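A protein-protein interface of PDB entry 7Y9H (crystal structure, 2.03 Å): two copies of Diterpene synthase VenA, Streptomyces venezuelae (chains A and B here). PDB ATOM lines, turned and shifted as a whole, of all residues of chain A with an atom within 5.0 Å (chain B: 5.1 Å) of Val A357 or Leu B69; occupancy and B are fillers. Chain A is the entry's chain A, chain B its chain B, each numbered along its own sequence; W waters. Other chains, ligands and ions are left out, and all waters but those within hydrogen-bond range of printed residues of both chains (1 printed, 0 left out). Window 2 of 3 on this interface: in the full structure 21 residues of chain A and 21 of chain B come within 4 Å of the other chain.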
ATOM      1  N   ARG A 253       9.144   0.955 -17.835  1.00  0.00           N
ATOM      2  CA  ARG A 253      10.471   1.620 -17.935  1.00  0.00           C
ATOM      3  C   ARG A 253      10.860   1.688 -19.402  1.00  0.00           C
ATOM      4  O   ARG A 253      11.348   2.727 -19.841  1.00  0.00           O
ATOM      5  CB  ARG A 253      11.513   0.884 -17.088  1.00  0.00           C
ATOM      6  CG  ARG A 253      12.891   1.497 -17.187  1.00  0.00           C
ATOM      7  CD  ARG A 253      13.948   0.773 -16.400  1.00  0.00           C
ATOM      8  NE  ARG A 253      15.033   0.713 -17.352  1.00  0.00           N
ATOM      9  CZ  ARG A 253      15.863   1.710 -17.586  1.00  0.00           C
ATOM     10  NH1 ARG A 253      16.798   1.559 -18.516  1.00  0.00           N
ATOM     11  NH2 ARG A 253      15.771   2.843 -16.895  1.00  0.00           N
ATOM     12  N   PHE A 337      15.309  -3.899 -17.853  1.00  0.00           N
ATOM     13  CA  PHE A 337      16.098  -3.139 -16.849  1.00  0.00           C
ATOM     14  C   PHE A 337      17.307  -2.513 -17.541  1.00  0.00           C
ATOM     15  O   PHE A 337      18.094  -1.842 -16.867  1.00  0.00           O
ATOM     16  CB  PHE A 337      16.382  -4.012 -15.626  1.00  0.00           C
ATOM     17  CG  PHE A 337      15.123  -4.238 -14.829  1.00  0.00           C
ATOM     18  CD1 PHE A 337      14.733  -3.354 -13.848  1.00  0.00           C
ATOM     19  CD2 PHE A 337      14.277  -5.305 -15.139  1.00  0.00           C
ATOM     20  CE1 PHE A 337      13.527  -3.526 -13.176  1.00  0.00           C
ATOM     21  CE2 PHE A 337      13.080  -5.480 -14.465  1.00  0.00           C
ATOM     22  CZ  PHE A 337      12.703  -4.582 -13.498  1.00  0.00           C
ATOM     23  N   GLY A 338      17.437  -2.730 -18.847  1.00  0.00           N
ATOM     24  CA  GLY A 338      18.458  -2.080 -19.696  1.00  0.00           C
ATOM     25  C   GLY A 338      19.628  -3.021 -20.006  1.00  0.00           C
ATOM     26  O   GLY A 338      19.988  -3.918 -19.183  1.00  0.00           O
ATOM     27  N   ASP A 339      20.179  -2.871 -21.193  1.00  0.00           N
ATOM     28  CA  ASP A 339      21.350  -3.639 -21.631  1.00  0.00           C
ATOM     29  C   ASP A 339      22.477  -3.393 -20.612  1.00  0.00           C
ATOM     30  O   ASP A 339      22.746  -2.241 -20.296  1.00  0.00           O
ATOM     31  CB  ASP A 339      21.723  -3.262 -23.053  1.00  0.00           C
ATOM     32  CG  ASP A 339      22.796  -4.152 -23.598  1.00  0.00           C
ATOM     33  OD1 ASP A 339      22.715  -5.373 -23.338  1.00  0.00           O
ATOM     34  OD2 ASP A 339      23.689  -3.625 -24.283  1.00  0.00           O
ATOM     35  N   GLY A 340      23.106  -4.459 -20.136  1.00  0.00           N
ATOM     36  CA  GLY A 340      24.195  -4.422 -19.149  1.00  0.00           C
ATOM     37  C   GLY A 340      23.707  -4.661 -17.746  1.00  0.00           C
ATOM     38  O   GLY A 340      24.553  -4.883 -16.885  1.00  0.00           O
ATOM     39  N   SER A 341      22.391  -4.533 -17.490  1.00  0.00           N
ATOM     40  CA  SER A 341      21.786  -4.859 -16.178  1.00  0.00           C
ATOM     41  C   SER A 341      22.046  -6.336 -15.838  1.00  0.00           C
ATOM     42  O   SER A 341      22.154  -7.159 -16.744  1.00  0.00           O
ATOM     43  CB  SER A 341      20.294  -4.512 -16.119  1.00  0.00           C
ATOM     44  OG  SER A 341      19.563  -5.164 -17.149  1.00  0.00           O
ATOM     45  N   VAL A 342      22.124  -6.615 -14.554  1.00  0.00           N
ATOM     46  CA  VAL A 342      22.245  -7.965 -13.964  1.00  0.00           C
ATOM     47  C   VAL A 342      21.391  -7.973 -12.711  1.00  0.00           C
ATOM     48  O   VAL A 342      21.679  -7.217 -11.769  1.00  0.00           O
ATOM     49  CB  VAL A 342      23.693  -8.348 -13.626  1.00  0.00           C
ATOM     50  CG1 VAL A 342      23.707  -9.765 -13.103  1.00  0.00           C
ATOM     51  CG2 VAL A 342      24.612  -8.180 -14.836  1.00  0.00           C
ATOM     52  N   ALA A 355      17.611   6.328 -16.294  1.00  0.00           N
ATOM     53  CA  ALA A 355      18.913   5.619 -16.268  1.00  0.00           C
ATOM     54  C   ALA A 355      19.039   4.677 -17.472  1.00  0.00           C
ATOM     55  O   ALA A 355      18.021   4.100 -17.909  1.00  0.00           O
ATOM     56  CB  ALA A 355      19.061   4.879 -14.971  1.00  0.00           C
ATOM     57  N   SER A 356      20.262   4.437 -17.950  1.00  0.00           N
ATOM     58  CA  SER A 356      20.549   3.455 -19.018  1.00  0.00           C
ATOM     59  C   SER A 356      20.433   2.027 -18.436  1.00  0.00           C
ATOM     60  O   SER A 356      20.161   1.080 -19.208  1.00  0.00           O
ATOM     61  CB  SER A 356      21.901   3.710 -19.651  1.00  0.00           C
ATOM     62  OG  SER A 356      22.931   3.664 -18.670  1.00  0.00           O
ATOM     63  N   VAL A 357      20.653   1.845 -17.135  1.00  0.00           N
ATOM     64  CA  VAL A 357      20.382   0.562 -16.425  1.00  0.00           C
ATOM     65  C   VAL A 357      19.625   0.885 -15.146  1.00  0.00           C
ATOM     66  O   VAL A 357      19.925   1.875 -14.472  1.00  0.00           O
ATOM     67  CB  VAL A 357      21.658  -0.247 -16.114  1.00  0.00           C
ATOM     68  CG1 VAL A 357      22.267  -0.825 -17.368  1.00  0.00           C
ATOM     69  CG2 VAL A 357      22.686   0.594 -15.372  1.00  0.00           C
ATOM     70  N   ALA A 358      18.707   0.013 -14.777  1.00  0.00           N
ATOM     71  CA  ALA A 358      17.836   0.214 -13.612  1.00  0.00           C
ATOM     72  C   ALA A 358      17.786  -1.051 -12.758  1.00  0.00           C
ATOM     73  O   ALA A 358      17.970  -2.169 -13.309  1.00  0.00           O
ATOM     74  CB  ALA A 358      16.463   0.622 -14.080  1.00  0.00           C
ATOM     75  N   ARG A 359      17.535  -0.841 -11.469  1.00  0.00           N
ATOM     76  CA  ARG A 359      17.293  -1.876 -10.424  1.00  0.00           C
ATOM     77  C   ARG A 359      16.463  -1.185  -9.354  1.00  0.00           C
ATOM     78  O   ARG A 359      16.489   0.059  -9.331  1.00  0.00           O
ATOM     79  CB  ARG A 359      18.584  -2.401  -9.791  1.00  0.00           C
ATOM     80  CG  ARG A 359      19.383  -1.346  -9.040  1.00  0.00           C
ATOM     81  CD  ARG A 359      20.798  -1.822  -8.740  1.00  0.00           C
ATOM     82  NE  ARG A 359      21.580  -0.782  -8.082  1.00  0.00           N
ATOM     83  CZ  ARG A 359      21.513  -0.468  -6.790  1.00  0.00           C
ATOM     84  NH1 ARG A 359      20.722  -1.138  -5.967  1.00  0.00           N
ATOM     85  NH2 ARG A 359      22.271   0.510  -6.314  1.00  0.00           N
ATOM     86  N   ARG B  55      26.355  -7.764  -4.490  1.00  0.00           N
ATOM     87  CA  ARG B  55      25.905  -6.361  -4.313  1.00  0.00           C
ATOM     88  C   ARG B  55      25.901  -6.022  -2.816  1.00  0.00           C
ATOM     89  O   ARG B  55      26.480  -4.996  -2.437  1.00  0.00           O
ATOM     90  CB  ARG B  55      24.508  -6.100  -4.879  1.00  0.00           C
ATOM     91  CG  ARG B  55      24.005  -4.695  -4.566  1.00  0.00           C
ATOM     92  CD  ARG B  55      22.692  -4.369  -5.249  1.00  0.00           C
ATOM     93  NE  ARG B  55      22.812  -4.420  -6.694  1.00  0.00           N
ATOM     94  CZ  ARG B  55      23.486  -3.565  -7.419  1.00  0.00           C
ATOM     95  NH1 ARG B  55      24.106  -2.553  -6.846  1.00  0.00           N
ATOM     96  NH2 ARG B  55      23.529  -3.705  -8.730  1.00  0.00           N
ATOM     97  N   GLU B  65      28.566   1.569  -9.997  1.00  0.00           N
ATOM     98  CA  GLU B  65      27.575   0.604 -10.517  1.00  0.00           C
ATOM     99  C   GLU B  65      28.110  -0.027 -11.813  1.00  0.00           C
ATOM    100  O   GLU B  65      27.932  -1.231 -11.962  1.00  0.00           O
ATOM    101  CB  GLU B  65      26.218   1.310 -10.618  1.00  0.00           C
ATOM    102  CG  GLU B  65      25.084   0.386 -10.980  1.00  0.00           C
ATOM    103  CD  GLU B  65      24.680  -0.660  -9.951  1.00  0.00           C
ATOM    104  OE1 GLU B  65      25.162  -0.617  -8.809  1.00  0.00           O
ATOM    105  OE2 GLU B  65      23.854  -1.523 -10.309  1.00  0.00           O
ATOM    106  N   GLU B  66      28.785   0.724 -12.686  1.00  0.00           N
ATOM    107  CA  GLU B  66      29.250   0.247 -14.018  1.00  0.00           C
ATOM    108  C   GLU B  66      30.200  -0.936 -13.793  1.00  0.00           C
ATOM    109  O   GLU B  66      30.077  -1.949 -14.520  1.00  0.00           O
ATOM    110  CB  GLU B  66      29.967   1.346 -14.829  1.00  0.00           C
ATOM    111  CG  GLU B  66      30.781   0.866 -16.050  1.00  0.00           C
ATOM    112  CD  GLU B  66      32.280   0.558 -15.910  1.00  0.00           C
ATOM    113  OE1 GLU B  66      32.761  -0.474 -16.509  1.00  0.00           O
ATOM    114  OE2 GLU B  66      32.991   1.343 -15.237  1.00  0.00           O
ATOM    115  N   SER B  67      31.147  -0.754 -12.867  1.00  0.00           N
ATOM    116  CA  SER B  67      32.246  -1.691 -12.569  1.00  0.00           C
ATOM    117  C   SER B  67      31.660  -2.942 -11.922  1.00  0.00           C
ATOM    118  O   SER B  67      32.020  -4.043 -12.331  1.00  0.00           O
ATOM    119  CB  SER B  67      33.286  -1.030 -11.683  1.00  0.00           C
ATOM    120  OG  SER B  67      34.323  -0.547 -12.493  1.00  0.00           O
ATOM    121  N   LEU B  68      30.746  -2.761 -10.977  1.00  0.00           N
ATOM    122  CA  LEU B  68      30.017  -3.897 -10.344  1.00  0.00           C
ATOM    123  C   LEU B  68      29.289  -4.707 -11.422  1.00  0.00           C
ATOM    124  O   LEU B  68      29.459  -5.949 -11.468  1.00  0.00           O
ATOM    125  CB  LEU B  68      29.057  -3.362  -9.283  1.00  0.00           C
ATOM    126  CG  LEU B  68      28.111  -4.406  -8.692  1.00  0.00           C
ATOM    127  CD1 LEU B  68      28.904  -5.523  -8.032  1.00  0.00           C
ATOM    128  CD2 LEU B  68      27.185  -3.759  -7.692  1.00  0.00           C
ATOM    129  N   LEU B  69      28.521  -4.058 -12.297  1.00  0.00           N
ATOM    130  CA  LEU B  69      27.733  -4.782 -13.325  1.00  0.00           C
ATOM    131  C   LEU B  69      28.673  -5.461 -14.314  1.00  0.00           C
ATOM    132  O   LEU B  69      28.306  -6.548 -14.780  1.00  0.00           O
ATOM    133  CB  LEU B  69      26.776  -3.853 -14.058  1.00  0.00           C
ATOM    134  CG  LEU B  69      25.663  -3.275 -13.195  1.00  0.00           C
ATOM    135  CD1 LEU B  69      24.810  -2.316 -13.996  1.00  0.00           C
ATOM    136  CD2 LEU B  69      24.804  -4.376 -12.612  1.00  0.00           C
ATOM    137  N   PHE B  70      29.780  -4.811 -14.676  1.00  0.00           N
ATOM    138  CA  PHE B  70      30.812  -5.415 -15.546  1.00  0.00           C
ATOM    139  C   PHE B  70      31.233  -6.767 -14.936  1.00  0.00           C
ATOM    140  O   PHE B  70      31.292  -7.815 -15.626  1.00  0.00           O
ATOM    141  CB  PHE B  70      31.998  -4.455 -15.698  1.00  0.00           C
ATOM    142  CG  PHE B  70      33.171  -5.040 -16.424  1.00  0.00           C
ATOM    143  CD1 PHE B  70      34.150  -5.727 -15.742  1.00  0.00           C
ATOM    144  CD2 PHE B  70      33.270  -4.928 -17.807  1.00  0.00           C
ATOM    145  CE1 PHE B  70      35.213  -6.298 -16.430  1.00  0.00           C
ATOM    146  CE2 PHE B  70      34.346  -5.479 -18.494  1.00  0.00           C
ATOM    147  CZ  PHE B  70      35.313  -6.177 -17.796  1.00  0.00           C
ATOM    148  N   PHE B  71      31.546  -6.740 -13.646  1.00  0.00           N
ATOM    149  CA  PHE B  71      31.880  -7.962 -12.883  1.00  0.00           C
ATOM    150  C   PHE B  71      30.711  -8.953 -12.891  1.00  0.00           C
ATOM    151  O   PHE B  71      30.933 -10.138 -13.187  1.00  0.00           O
ATOM    152  CB  PHE B  71      32.323  -7.593 -11.464  1.00  0.00           C
ATOM    153  CG  PHE B  71      32.630  -8.836 -10.685  1.00  0.00           C
ATOM    154  CD1 PHE B  71      33.821  -9.513 -10.907  1.00  0.00           C
ATOM    155  CD2 PHE B  71      31.693  -9.377  -9.829  1.00  0.00           C
ATOM    156  CE1 PHE B  71      34.073 -10.692 -10.236  1.00  0.00           C
ATOM    157  CE2 PHE B  71      31.943 -10.565  -9.173  1.00  0.00           C
ATOM    158  CZ  PHE B  71      33.131 -11.206  -9.368  1.00  0.00           C
ATOM    159  N   LEU B  72      29.486  -8.514 -12.546  1.00  0.00           N
ATOM    160  CA  LEU B  72      28.326  -9.445 -12.490  1.00  0.00           C
ATOM    161  C   LEU B  72      28.075 -10.049 -13.879  1.00  0.00           C
ATOM    162  O   LEU B  72      27.622 -11.231 -13.941  1.00  0.00           O
ATOM    163  CB  LEU B  72      27.079  -8.761 -11.905  1.00  0.00           C
ATOM    164  CG  LEU B  72      27.246  -8.216 -10.492  1.00  0.00           C
ATOM    165  CD1 LEU B  72      25.988  -7.482 -10.045  1.00  0.00           C
ATOM    166  CD2 LEU B  72      27.605  -9.314  -9.507  1.00  0.00           C
ATOM    167  N   ARG B  73      28.406  -9.340 -14.962  1.00  0.00           N
ATOM    168  CA  ARG B  73      28.139  -9.835 -16.343  1.00  0.00           C
ATOM    169  C   ARG B  73      29.067 -11.015 -16.654  1.00  0.00           C
ATOM    170  O   ARG B  73      28.750 -11.764 -17.598  1.00  0.00           O
ATOM    171  CB  ARG B  73      28.232  -8.719 -17.390  1.00  0.00           C
ATOM    172  CG  ARG B  73      27.021  -7.790 -17.394  1.00  0.00           C
ATOM    173  CD  ARG B  73      26.941  -6.964 -18.656  1.00  0.00           C
ATOM    174  NE  ARG B  73      28.075  -6.065 -18.839  1.00  0.00           N
ATOM    175  CZ  ARG B  73      28.201  -4.866 -18.288  1.00  0.00           C
ATOM    176  NH1 ARG B  73      27.298  -4.412 -17.442  1.00  0.00           N
ATOM    177  NH2 ARG B  73      29.276  -4.140 -18.539  1.00  0.00           N
HETATM  178  O   HOH W   1      21.532  -5.443 -10.059  1.00  0.00           O
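The guanidinium group of Arg B73 is in hydrogen-bond range of the backbone carbonyl oxygen of Gly A340 (2.8 Å).
The guanidinium group (NE) of Arg A359 is in salt-bridge range of the side-chain carboxylate (OE2) of Glu B65 (3.3 Å).
The guanidinium group of Arg B55 lies close to the guanidinium group of Arg A359 (3.3 Å).
NH2 of Arg B55 is in salt-bridge range of OE2 of Glu B65, 2.7 Å away.
Gly A340 touches Leu B69.
N of Val A342 touches CD2 of Leu B69 (3.996 Å).
CG1 of Val A342 touches CB of Leu B72, at 3.7 Å.
CG2 of Val A342 touches CG of Arg B73, 3.5 Å away.
Leu B69 touches Val A357 (CD1 to CG2, 3.9 Å).
Of chain B, only Leu B69 comes within 4 Å of Val A357.
Printed residues of chain A within 4 Å of Leu B69: Gly A340, Val A342 and Val A357.
Printed residues of chain B within 4 Å of Val A342: Leu B69, Leu B72 and Arg B73.
Printed residues of chain A within 4 Å of Arg B73: Gly A340 and Val A342.
Of the printed residues of chain A, Arg B55 touches Arg A359.
Of the printed residues of chain A, Glu B65 touches Arg A359 (3.3 Å).
Printed residues of chain B within 4 Å of Gly A340: Leu B69 and Arg B73.
Glu B66 touches none of the printed residues of chain A.
The nearest residue of chain B that does not touch Val A357 is Glu B65 (5.0 Å).
The nearest printed residue of chain A that does not touch Leu B69 is Ser A341 (4.5 Å).
The nearest printed residue of chain B that does not touch Val A342 is Arg B55 (5.0 Å).
Of the 10 printed residues of chain B, 5 touch a printed residue of chain A.
Of the 12 printed residues of chain A, 4 touch a printed residue of chain B.
Printed residues of chain A that touch a printed residue of chain B: Gly A340, Val A342, Val A357 and Arg A359.
Hydrophobic or aromatic side chains of chain A within 4 Å of the printed part of chain B: Val A342 and Val A357.
Among the printed residues, Asp or Glu carboxylates within 4 Å of a Lys or Arg side-chain nitrogen of the other chain: Arg A359 with Glu B65 (3.3 Å).
No position is printed for both chains.
Of the 8 pairs that touch across the chains among the printed residues, none has its exchanged pair printed and touching as well.
Water W1 bridges the backbone carbonyl oxygen (O) of Val A342 (2.5 Å) and the guanidinium group (NH2) of Arg B55 (3.0 Å).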
